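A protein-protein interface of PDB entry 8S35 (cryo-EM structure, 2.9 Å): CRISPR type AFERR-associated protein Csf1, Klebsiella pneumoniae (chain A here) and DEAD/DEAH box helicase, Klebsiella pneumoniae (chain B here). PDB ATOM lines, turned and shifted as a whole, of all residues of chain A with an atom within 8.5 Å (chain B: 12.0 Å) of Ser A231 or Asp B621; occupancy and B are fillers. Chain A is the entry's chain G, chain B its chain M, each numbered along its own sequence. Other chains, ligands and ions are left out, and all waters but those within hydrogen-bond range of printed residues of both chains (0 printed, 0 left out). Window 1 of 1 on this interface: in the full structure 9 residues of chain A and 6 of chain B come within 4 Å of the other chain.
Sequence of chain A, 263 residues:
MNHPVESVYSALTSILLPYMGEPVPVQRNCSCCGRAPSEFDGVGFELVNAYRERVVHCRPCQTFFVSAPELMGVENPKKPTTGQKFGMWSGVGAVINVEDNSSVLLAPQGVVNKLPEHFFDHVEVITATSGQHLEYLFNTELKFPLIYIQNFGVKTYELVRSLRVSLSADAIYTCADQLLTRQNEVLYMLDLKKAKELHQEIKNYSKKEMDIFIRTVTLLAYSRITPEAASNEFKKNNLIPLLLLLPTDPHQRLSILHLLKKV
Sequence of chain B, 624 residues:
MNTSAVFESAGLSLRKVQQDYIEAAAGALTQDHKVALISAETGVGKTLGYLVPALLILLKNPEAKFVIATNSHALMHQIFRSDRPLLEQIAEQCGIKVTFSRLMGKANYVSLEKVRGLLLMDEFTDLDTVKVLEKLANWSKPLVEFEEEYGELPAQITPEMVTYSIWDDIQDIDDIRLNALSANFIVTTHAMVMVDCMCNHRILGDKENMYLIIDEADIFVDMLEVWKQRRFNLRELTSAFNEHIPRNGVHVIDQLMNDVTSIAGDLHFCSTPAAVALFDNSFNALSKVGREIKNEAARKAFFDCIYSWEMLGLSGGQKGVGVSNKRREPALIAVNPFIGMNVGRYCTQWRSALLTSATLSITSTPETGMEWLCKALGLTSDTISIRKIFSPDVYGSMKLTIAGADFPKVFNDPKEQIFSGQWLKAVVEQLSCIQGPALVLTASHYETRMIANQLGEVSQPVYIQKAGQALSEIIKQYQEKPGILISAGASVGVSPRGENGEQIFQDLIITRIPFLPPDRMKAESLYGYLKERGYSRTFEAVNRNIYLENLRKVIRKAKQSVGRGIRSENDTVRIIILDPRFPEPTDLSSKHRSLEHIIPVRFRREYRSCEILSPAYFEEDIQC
N of Glu A228 is in hydrogen-bond range of OD2 of Asp B621 (3.4 Å). The side-chain carboxylate (OE1) of Glu A228 lies close to the side-chain carboxylate (OE2) of Glu B619.
The side-chain hydroxyl (OG) of Ser A231 sits at hydrogen-bond distance from the backbone carbonyl oxygen (O) of Pro A227 (3.2 Å). O of Glu A228 sits at hydrogen-bond distance from OG of Ser A231. O of Glu A228 lies close to OD1 of Asn A232 (3.1 Å). The backbone carbonyl oxygen of Phe A234 is in hydrogen-bond range of the backbone NH of Leu A239 (2.7 Å). The side-chain sulfur (SG) of Cys B624 is in hydrogen-bond range of the backbone carbonyl oxygen (O) of Asp B621 (3.1 Å). The backbone carbonyl oxygen (O) of Ile B622 is in hydrogen-bond range of the side-chain sulfur (SG) of Cys B624 (3.4 Å).
Among the printed residues, pairs that only touch across the chains: Glu A228 with Tyr B617 (3.2 Å), Leu A220 with Gln B623 (3.3 Å), Leu A243 with Ile B622 (3.5 Å), Pro A227 with Asp B621 (3.5 Å), Ile A240 with Ile B622 (3.5 Å), Pro A227 with Gln B623 (3.6 Å), Ser A231 with Ile B622 (3.7 Å), Leu A243 with Gln B623 (3.8 Å), Phe A234 with Ile B622 (3.9 Å), Ser A231 with Asp B621 (3.9 Å) and Lys A235 with Glu B620 (3.96 Å).
Printed residues of chain B within 4 Å of Ser A231: Asp B621 and Ile B622. Of the printed residues of chain A, Asp B621 touches Pro A227, Glu A228 and Ser A231. Of the printed residues of chain B, Pro A227 touches Asp B621 and Gln B623. Of chain B, only Tyr B617, Glu B619 and Asp B621 come within 4 Å of Glu A228. No residue of chain B comes within 4 Å of Ala A229. No residue of chain B comes within 4 Å of Ala A230. No residue of chain B comes within 4 Å of Asn A232. Of chain B, only Ile B622 (3.9 Å) comes within 4 Å of Phe A234. Of chain B, only Glu B620 comes within 4 Å of Lys A235. Of the printed residues of chain A, Tyr B617 touches Glu A228 (3.2 Å). Of the printed residues of chain B, Leu A220 touches Gln B623. The nearest residue of chain B that does not touch Ser A231 is Gln B623 (4.9 Å). The nearest residue of chain A that does not touch Asp B621 is Lys A235 (5.3 Å).
Of the 19 printed residues of chain A, 8 touch a printed residue of chain B. Of the 12 printed residues of chain B, 6 touch a printed residue of chain A. Printed residues of chain B that touch a printed residue of chain A: Tyr B617, Glu B619, Glu B620, Asp B621, Ile B622 and Gln B623. Hydrophobic or aromatic side chains of chain B within 4 Å of the printed part of chain A: Tyr B617 and Ile B622. Among the printed residues, 13 pairs touch across the chains.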
ATOM      1  N   THR A 216      22.931  -6.267 -23.520  1.00  0.00           N
ATOM      2  CA  THR A 216      22.285  -6.492 -22.234  1.00  0.00           C
ATOM      3  C   THR A 216      22.754  -5.475 -21.204  1.00  0.00           C
ATOM      4  O   THR A 216      21.942  -4.888 -20.479  1.00  0.00           O
ATOM      5  CB  THR A 216      22.571  -7.914 -21.752  1.00  0.00           C
ATOM      6  OG1 THR A 216      22.269  -8.847 -22.796  1.00  0.00           O
ATOM      7  CG2 THR A 216      21.739  -8.249 -20.525  1.00  0.00           C
ATOM      8  N   LEU A 220      20.504  -2.585 -19.436  1.00  0.00           N
ATOM      9  CA  LEU A 220      20.406  -2.564 -17.982  1.00  0.00           C
ATOM     10  C   LEU A 220      20.841  -1.215 -17.426  1.00  0.00           C
ATOM     11  O   LEU A 220      20.177  -0.653 -16.547  1.00  0.00           O
ATOM     12  CB  LEU A 220      21.252  -3.690 -17.390  1.00  0.00           C
ATOM     13  CG  LEU A 220      21.107  -3.969 -15.894  1.00  0.00           C
ATOM     14  CD1 LEU A 220      19.686  -4.390 -15.538  1.00  0.00           C
ATOM     15  CD2 LEU A 220      22.110  -5.033 -15.473  1.00  0.00           C
ATOM     16  N   ILE A 225      15.794  -3.111 -19.586  1.00  0.00           N
ATOM     17  CA  ILE A 225      15.491  -4.505 -19.290  1.00  0.00           C
ATOM     18  C   ILE A 225      15.591  -4.698 -17.786  1.00  0.00           C
ATOM     19  O   ILE A 225      16.433  -4.078 -17.125  1.00  0.00           O
ATOM     20  CB  ILE A 225      16.436  -5.476 -20.029  1.00  0.00           C
ATOM     21  CG1 ILE A 225      17.902  -5.172 -19.697  1.00  0.00           C
ATOM     22  CG2 ILE A 225      16.189  -5.402 -21.528  1.00  0.00           C
ATOM     23  CD1 ILE A 225      18.877  -6.136 -20.326  1.00  0.00           C
ATOM     24  N   THR A 226      14.733  -5.554 -17.245  1.00  0.00           N
ATOM     25  CA  THR A 226      14.745  -5.797 -15.816  1.00  0.00           C
ATOM     26  C   THR A 226      16.041  -6.503 -15.417  1.00  0.00           C
ATOM     27  O   THR A 226      16.630  -7.229 -16.221  1.00  0.00           O
ATOM     28  CB  THR A 226      13.548  -6.650 -15.409  1.00  0.00           C
ATOM     29  OG1 THR A 226      13.672  -7.953 -15.989  1.00  0.00           O
ATOM     30  CG2 THR A 226      12.249  -6.010 -15.879  1.00  0.00           C
ATOM     31  N   PRO A 227      16.520  -6.298 -14.183  1.00  0.00           N
ATOM     32  CA  PRO A 227      17.727  -7.019 -13.754  1.00  0.00           C
ATOM     33  C   PRO A 227      17.603  -8.525 -13.846  1.00  0.00           C
ATOM     34  O   PRO A 227      18.603  -9.201 -14.115  1.00  0.00           O
ATOM     35  CB  PRO A 227      17.906  -6.556 -12.304  1.00  0.00           C
ATOM     36  CG  PRO A 227      17.332  -5.214 -12.297  1.00  0.00           C
ATOM     37  CD  PRO A 227      16.123  -5.298 -13.178  1.00  0.00           C
ATOM     38  N   GLU A 228      16.411  -9.080 -13.625  1.00  0.00           N
ATOM     39  CA  GLU A 228      16.250 -10.523 -13.754  1.00  0.00           C
ATOM     40  C   GLU A 228      16.478 -10.966 -15.192  1.00  0.00           C
ATOM     41  O   GLU A 228      17.099 -12.005 -15.439  1.00  0.00           O
ATOM     42  CB  GLU A 228      14.866 -10.949 -13.263  1.00  0.00           C
ATOM     43  CG  GLU A 228      13.696 -10.328 -14.011  1.00  0.00           C
ATOM     44  CD  GLU A 228      12.357 -10.792 -13.477  1.00  0.00           C
ATOM     45  OE1 GLU A 228      12.343 -11.643 -12.563  1.00  0.00           O
ATOM     46  OE2 GLU A 228      11.318 -10.307 -13.973  1.00  0.00           O
ATOM     47  N   ALA A 229      16.004 -10.176 -16.157  1.00  0.00           N
ATOM     48  CA  ALA A 229      16.219 -10.518 -17.558  1.00  0.00           C
ATOM     49  C   ALA A 229      17.700 -10.474 -17.910  1.00  0.00           C
ATOM     50  O   ALA A 229      18.213 -11.375 -18.583  1.00  0.00           O
ATOM     51  CB  ALA A 229      15.426  -9.568 -18.456  1.00  0.00           C
ATOM     52  N   ALA A 230      18.401  -9.430 -17.467  1.00  0.00           N
ATOM     53  CA  ALA A 230      19.830  -9.338 -17.738  1.00  0.00           C
ATOM     54  C   ALA A 230      20.586 -10.484 -17.082  1.00  0.00           C
ATOM     55  O   ALA A 230      21.513 -11.047 -17.674  1.00  0.00           O
ATOM     56  CB  ALA A 230      20.370  -7.994 -17.256  1.00  0.00           C
ATOM     57  N   SER A 231      20.216 -10.833 -15.848  1.00  0.00           N
ATOM     58  CA  SER A 231      20.870 -11.947 -15.173  1.00  0.00           C
ATOM     59  C   SER A 231      20.630 -13.251 -15.917  1.00  0.00           C
ATOM     60  O   SER A 231      21.540 -14.076 -16.050  1.00  0.00           O
ATOM     61  CB  SER A 231      20.368 -12.050 -13.734  1.00  0.00           C
ATOM     62  OG  SER A 231      18.988 -12.368 -13.701  1.00  0.00           O
ATOM     63  N   ASN A 232      19.404 -13.460 -16.404  1.00  0.00           N
ATOM     64  CA  ASN A 232      19.119 -14.648 -17.200  1.00  0.00           C
ATOM     65  C   ASN A 232      19.969 -14.672 -18.460  1.00  0.00           C
ATOM     66  O   ASN A 232      20.510 -15.719 -18.834  1.00  0.00           O
ATOM     67  CB  ASN A 232      17.636 -14.696 -17.556  1.00  0.00           C
ATOM     68  CG  ASN A 232      16.752 -14.857 -16.339  1.00  0.00           C
ATOM     69  OD1 ASN A 232      17.237 -15.086 -15.232  1.00  0.00           O
ATOM     70  ND2 ASN A 232      15.445 -14.738 -16.539  1.00  0.00           N
ATOM     71  N   GLU A 233      20.097 -13.526 -19.130  1.00  0.00           N
ATOM     72  CA  GLU A 233      20.903 -13.471 -20.345  1.00  0.00           C
ATOM     73  C   GLU A 233      22.362 -13.789 -20.052  1.00  0.00           C
ATOM     74  O   GLU A 233      23.006 -14.534 -20.799  1.00  0.00           O
ATOM     75  CB  GLU A 233      20.776 -12.094 -20.993  1.00  0.00           C
ATOM     76  CG  GLU A 233      19.406 -11.810 -21.589  1.00  0.00           C
ATOM     77  CD  GLU A 233      19.125 -12.625 -22.836  1.00  0.00           C
ATOM     78  OE1 GLU A 233      20.082 -13.170 -23.424  1.00  0.00           O
ATOM     79  OE2 GLU A 233      17.943 -12.719 -23.229  1.00  0.00           O
ATOM     80  N   PHE A 234      22.902 -13.235 -18.965  1.00  0.00           N
ATOM     81  CA  PHE A 234      24.293 -13.504 -18.618  1.00  0.00           C
ATOM     82  C   PHE A 234      24.499 -14.971 -18.267  1.00  0.00           C
ATOM     83  O   PHE A 234      25.469 -15.592 -18.718  1.00  0.00           O
ATOM     84  CB  PHE A 234      24.733 -12.614 -17.454  1.00  0.00           C
ATOM     85  CG  PHE A 234      24.666 -11.138 -17.745  1.00  0.00           C
ATOM     86  CD1 PHE A 234      25.046 -10.632 -18.976  1.00  0.00           C
ATOM     87  CD2 PHE A 234      24.237 -10.253 -16.771  1.00  0.00           C
ATOM     88  CE1 PHE A 234      24.985  -9.279 -19.234  1.00  0.00           C
ATOM     89  CE2 PHE A 234      24.174  -8.899 -17.026  1.00  0.00           C
ATOM     90  CZ  PHE A 234      24.549  -8.412 -18.257  1.00  0.00           C
ATOM     91  N   LYS A 235      23.600 -15.543 -17.465  1.00  0.00           N
ATOM     92  CA  LYS A 235      23.750 -16.937 -17.064  1.00  0.00           C
ATOM     93  C   LYS A 235      23.634 -17.868 -18.261  1.00  0.00           C
ATOM     94  O   LYS A 235      24.412 -18.821 -18.395  1.00  0.00           O
ATOM     95  CB  LYS A 235      22.706 -17.288 -16.006  1.00  0.00           C
ATOM     96  CG  LYS A 235      22.984 -16.672 -14.646  1.00  0.00           C
ATOM     97  CD  LYS A 235      21.961 -17.109 -13.613  1.00  0.00           C
ATOM     98  CE  LYS A 235      20.637 -16.384 -13.794  1.00  0.00           C
ATOM     99  NZ  LYS A 235      19.703 -16.641 -12.663  1.00  0.00           N
ATOM    100  N   LYS A 236      22.669 -17.611 -19.145  1.00  0.00           N
ATOM    101  CA  LYS A 236      22.494 -18.468 -20.311  1.00  0.00           C
ATOM    102  C   LYS A 236      23.674 -18.361 -21.266  1.00  0.00           C
ATOM    103  O   LYS A 236      24.029 -19.349 -21.920  1.00  0.00           O
ATOM    104  CB  LYS A 236      21.196 -18.111 -21.033  1.00  0.00           C
ATOM    105  CG  LYS A 236      19.941 -18.402 -20.227  1.00  0.00           C
ATOM    106  CD  LYS A 236      18.753 -17.604 -20.741  1.00  0.00           C
ATOM    107  CE  LYS A 236      17.436 -18.101 -20.160  1.00  0.00           C
ATOM    108  NZ  LYS A 236      17.566 -18.583 -18.756  1.00  0.00           N
ATOM    109  N   ASN A 237      24.291 -17.185 -21.359  1.00  0.00           N
ATOM    110  CA  ASN A 237      25.438 -16.967 -22.227  1.00  0.00           C
ATOM    111  C   ASN A 237      26.769 -17.082 -21.495  1.00  0.00           C
ATOM    112  O   ASN A 237      27.815 -16.837 -22.104  1.00  0.00           O
ATOM    113  CB  ASN A 237      25.332 -15.593 -22.893  1.00  0.00           C
ATOM    114  CG  ASN A 237      24.347 -15.581 -24.041  1.00  0.00           C
ATOM    115  OD1 ASN A 237      24.727 -15.731 -25.201  1.00  0.00           O
ATOM    116  ND2 ASN A 237      23.071 -15.408 -23.723  1.00  0.00           N
ATOM    117  N   ASN A 238      26.762 -17.454 -20.214  1.00  0.00           N
ATOM    118  CA  ASN A 238      27.993 -17.643 -19.448  1.00  0.00           C
ATOM    119  C   ASN A 238      28.823 -16.363 -19.409  1.00  0.00           C
ATOM    120  O   ASN A 238      30.046 -16.388 -19.561  1.00  0.00           O
ATOM    121  CB  ASN A 238      28.813 -18.803 -20.016  1.00  0.00           C
ATOM    122  CG  ASN A 238      29.888 -19.281 -19.061  1.00  0.00           C
ATOM    123  OD1 ASN A 238      29.725 -19.218 -17.842  1.00  0.00           O
ATOM    124  ND2 ASN A 238      30.995 -19.760 -19.611  1.00  0.00           N
ATOM    125  N   LEU A 239      28.152 -15.232 -19.195  1.00  0.00           N
ATOM    126  CA  LEU A 239      28.786 -13.921 -19.164  1.00  0.00           C
ATOM    127  C   LEU A 239      29.055 -13.439 -17.743  1.00  0.00           C
ATOM    128  O   LEU A 239      29.247 -12.238 -17.528  1.00  0.00           O
ATOM    129  CB  LEU A 239      27.924 -12.902 -19.911  1.00  0.00           C
ATOM    130  CG  LEU A 239      27.579 -13.259 -21.358  1.00  0.00           C
ATOM    131  CD1 LEU A 239      26.454 -12.374 -21.870  1.00  0.00           C
ATOM    132  CD2 LEU A 239      28.808 -13.150 -22.245  1.00  0.00           C
ATOM    133  N   ILE A 240      29.073 -14.351 -16.772  1.00  0.00           N
ATOM    134  CA  ILE A 240      29.224 -13.948 -15.372  1.00  0.00           C
ATOM    135  C   ILE A 240      30.559 -13.254 -15.118  1.00  0.00           C
ATOM    136  O   ILE A 240      30.563 -12.191 -14.477  1.00  0.00           O
ATOM    137  CB  ILE A 240      29.000 -15.149 -14.444  1.00  0.00           C
ATOM    138  CG1 ILE A 240      27.645 -15.831 -14.707  1.00  0.00           C
ATOM    139  CG2 ILE A 240      29.099 -14.713 -12.993  1.00  0.00           C
ATOM    140  CD1 ILE A 240      26.424 -15.002 -14.351  1.00  0.00           C
ATOM    141  N   LEU A 243      30.538  -9.554 -16.170  1.00  0.00           N
ATOM    142  CA  LEU A 243      29.827  -8.695 -15.233  1.00  0.00           C
ATOM    143  C   LEU A 243      30.647  -8.484 -13.970  1.00  0.00           C
ATOM    144  O   LEU A 243      30.701  -7.371 -13.434  1.00  0.00           O
ATOM    145  CB  LEU A 243      28.463  -9.298 -14.902  1.00  0.00           C
ATOM    146  CG  LEU A 243      27.641  -8.597 -13.819  1.00  0.00           C
ATOM    147  CD1 LEU A 243      27.512  -7.109 -14.100  1.00  0.00           C
ATOM    148  CD2 LEU A 243      26.272  -9.234 -13.721  1.00  0.00           C
ATOM    149  N   GLU B 584       4.625  -8.666  -0.707  1.00  0.00           N
ATOM    150  CA  GLU B 584       5.768  -9.432  -0.251  1.00  0.00           C
ATOM    151  C   GLU B 584       6.760  -8.503   0.448  1.00  0.00           C
ATOM    152  O   GLU B 584       6.820  -7.310   0.140  1.00  0.00           O
ATOM    153  CB  GLU B 584       6.450 -10.138  -1.420  1.00  0.00           C
ATOM    154  CG  GLU B 584       5.845 -11.492  -1.761  1.00  0.00           C
ATOM    155  CD  GLU B 584       6.640 -12.242  -2.815  1.00  0.00           C
ATOM    156  OE1 GLU B 584       7.880 -12.105  -2.839  1.00  0.00           O
ATOM    157  OE2 GLU B 584       6.020 -12.969  -3.621  1.00  0.00           O
ATOM    158  N   THR B 586       9.982  -8.284   0.157  1.00  0.00           N
ATOM    159  CA  THR B 586      10.956  -7.772  -0.795  1.00  0.00           C
ATOM    160  C   THR B 586      10.328  -6.860  -1.840  1.00  0.00           C
ATOM    161  O   THR B 586      11.045  -6.062  -2.455  1.00  0.00           O
ATOM    162  CB  THR B 586      11.668  -8.931  -1.496  1.00  0.00           C
ATOM    163  OG1 THR B 586      10.731  -9.653  -2.305  1.00  0.00           O
ATOM    164  CG2 THR B 586      12.286  -9.875  -0.475  1.00  0.00           C
ATOM    165  N   PRO B 615       6.606 -17.412  -3.849  1.00  0.00           N
ATOM    166  CA  PRO B 615       7.339 -16.182  -4.157  1.00  0.00           C
ATOM    167  C   PRO B 615       7.617 -16.054  -5.646  1.00  0.00           C
ATOM    168  O   PRO B 615       7.826 -17.045  -6.349  1.00  0.00           O
ATOM    169  CB  PRO B 615       8.637 -16.330  -3.357  1.00  0.00           C
ATOM    170  CG  PRO B 615       8.802 -17.796  -3.171  1.00  0.00           C
ATOM    171  CD  PRO B 615       7.419 -18.360  -3.070  1.00  0.00           C
ATOM    172  N   ALA B 616       7.621 -14.813  -6.116  1.00  0.00           N
ATOM    173  CA  ALA B 616       7.951 -14.498  -7.496  1.00  0.00           C
ATOM    174  C   ALA B 616       9.397 -14.035  -7.582  1.00  0.00           C
ATOM    175  O   ALA B 616       9.942 -13.465  -6.634  1.00  0.00           O
ATOM    176  CB  ALA B 616       7.023 -13.415  -8.046  1.00  0.00           C
ATOM    177  N   TYR B 617      10.018 -14.283  -8.735  1.00  0.00           N
ATOM    178  CA  TYR B 617      11.399 -13.867  -8.966  1.00  0.00           C
ATOM    179  C   TYR B 617      12.325 -14.535  -7.953  1.00  0.00           C
ATOM    180  O   TYR B 617      13.272 -13.930  -7.447  1.00  0.00           O
ATOM    181  CB  TYR B 617      11.529 -12.340  -8.918  1.00  0.00           C
ATOM    182  CG  TYR B 617      10.357 -11.596  -9.534  1.00  0.00           C
ATOM    183  CD1 TYR B 617       9.868 -10.434  -8.954  1.00  0.00           C
ATOM    184  CD2 TYR B 617       9.773 -12.027 -10.721  1.00  0.00           C
ATOM    185  CE1 TYR B 617       8.804  -9.752  -9.512  1.00  0.00           C
ATOM    186  CE2 TYR B 617       8.711 -11.348 -11.285  1.00  0.00           C
ATOM    187  CZ  TYR B 617       8.235 -10.208 -10.679  1.00  0.00           C
ATOM    188  OH  TYR B 617       7.181  -9.522 -11.238  1.00  0.00           O
ATOM    189  N   PHE B 618      12.038 -15.803  -7.659  1.00  0.00           N
ATOM    190  CA  PHE B 618      12.727 -16.556  -6.612  1.00  0.00           C
ATOM    191  C   PHE B 618      14.014 -17.168  -7.167  1.00  0.00           C
ATOM    192  O   PHE B 618      14.179 -18.386  -7.269  1.00  0.00           O
ATOM    193  CB  PHE B 618      11.802 -17.623  -6.043  1.00  0.00           C
ATOM    194  CG  PHE B 618      12.284 -18.216  -4.752  1.00  0.00           C
ATOM    195  CD1 PHE B 618      12.275 -17.470  -3.586  1.00  0.00           C
ATOM    196  CD2 PHE B 618      12.746 -19.519  -4.704  1.00  0.00           C
ATOM    197  CE1 PHE B 618      12.718 -18.012  -2.396  1.00  0.00           C
ATOM    198  CE2 PHE B 618      13.190 -20.068  -3.517  1.00  0.00           C
ATOM    199  CZ  PHE B 618      13.175 -19.314  -2.361  1.00  0.00           C
ATOM    200  N   GLU B 619      14.942 -16.285  -7.536  1.00  0.00           N
ATOM    201  CA  GLU B 619      16.245 -16.693  -8.044  1.00  0.00           C
ATOM    202  C   GLU B 619      17.301 -15.751  -7.482  1.00  0.00           C
ATOM    203  O   GLU B 619      16.996 -14.808  -6.744  1.00  0.00           O
ATOM    204  CB  GLU B 619      16.264 -16.708  -9.579  1.00  0.00           C
ATOM    205  CG  GLU B 619      15.828 -15.401 -10.241  1.00  0.00           C
ATOM    206  CD  GLU B 619      14.325 -15.301 -10.448  1.00  0.00           C
ATOM    207  OE1 GLU B 619      13.592 -16.231 -10.048  1.00  0.00           O
ATOM    208  OE2 GLU B 619      13.876 -14.285 -11.019  1.00  0.00           O
ATOM    209  N   GLU B 620      18.556 -16.012  -7.839  1.00  0.00           N
ATOM    210  CA  GLU B 620      19.708 -15.254  -7.353  1.00  0.00           C
ATOM    211  C   GLU B 620      20.278 -14.458  -8.522  1.00  0.00           C
ATOM    212  O   GLU B 620      21.052 -14.984  -9.326  1.00  0.00           O
ATOM    213  CB  GLU B 620      20.760 -16.178  -6.742  1.00  0.00           C
ATOM    214  CG  GLU B 620      21.053 -17.443  -7.543  1.00  0.00           C
ATOM    215  CD  GLU B 620      20.142 -18.597  -7.172  1.00  0.00           C
ATOM    216  OE1 GLU B 620      19.016 -18.336  -6.699  1.00  0.00           O
ATOM    217  OE2 GLU B 620      20.553 -19.761  -7.353  1.00  0.00           O
ATOM    218  N   ASP B 621      19.890 -13.189  -8.614  1.00  0.00           N
ATOM    219  CA  ASP B 621      20.405 -12.339  -9.676  1.00  0.00           C
ATOM    220  C   ASP B 621      21.912 -12.179  -9.532  1.00  0.00           C
ATOM    221  O   ASP B 621      22.472 -12.308  -8.441  1.00  0.00           O
ATOM    222  CB  ASP B 621      19.726 -10.972  -9.643  1.00  0.00           C
ATOM    223  CG  ASP B 621      18.273 -11.035 -10.058  1.00  0.00           C
ATOM    224  OD1 ASP B 621      17.600 -12.028  -9.711  1.00  0.00           O
ATOM    225  OD2 ASP B 621      17.804 -10.096 -10.734  1.00  0.00           O
ATOM    226  N   ILE B 622      22.568 -11.892 -10.657  1.00  0.00           N
ATOM    227  CA  ILE B 622      24.015 -11.715 -10.677  1.00  0.00           C
ATOM    228  C   ILE B 622      24.406 -10.241 -10.649  1.00  0.00           C
ATOM    229  O   ILE B 622      25.510  -9.916 -10.187  1.00  0.00           O
ATOM    230  CB  ILE B 622      24.633 -12.429 -11.904  1.00  0.00           C
ATOM    231  CG1 ILE B 622      26.171 -12.381 -11.874  1.00  0.00           C
ATOM    232  CG2 ILE B 622      24.077 -11.866 -13.218  1.00  0.00           C
ATOM    233  CD1 ILE B 622      26.791 -13.218 -10.771  1.00  0.00           C
ATOM    234  N   GLN B 623      23.534  -9.342 -11.107  1.00  0.00           N
ATOM    235  CA  GLN B 623      23.805  -7.907 -11.062  1.00  0.00           C
ATOM    236  C   GLN B 623      23.504  -7.361  -9.664  1.00  0.00           C
ATOM    237  O   GLN B 623      22.629  -6.522  -9.457  1.00  0.00           O
ATOM    238  CB  GLN B 623      22.986  -7.186 -12.123  1.00  0.00           C
ATOM    239  CG  GLN B 623      23.360  -5.714 -12.287  1.00  0.00           C
ATOM    240  CD  GLN B 623      22.187  -4.755 -12.128  1.00  0.00           C
ATOM    241  OE1 GLN B 623      21.109  -5.125 -11.662  1.00  0.00           O
ATOM    242  NE2 GLN B 623      22.399  -3.505 -12.521  1.00  0.00           N
ATOM    243  N   CYS B 624      24.261  -7.862  -8.693  1.00  0.00           N
ATOM    244  CA  CYS B 624      24.098  -7.465  -7.302  1.00  0.00           C
ATOM    245  C   CYS B 624      24.887  -6.191  -7.019  1.00  0.00           C
ATOM    246  O   CYS B 624      25.613  -6.099  -6.029  1.00  0.00           O
ATOM    247  CB  CYS B 624      24.547  -8.594  -6.370  1.00  0.00           C
ATOM    248  SG  CYS B 624      24.280 -10.249  -7.041  1.00  0.00           S
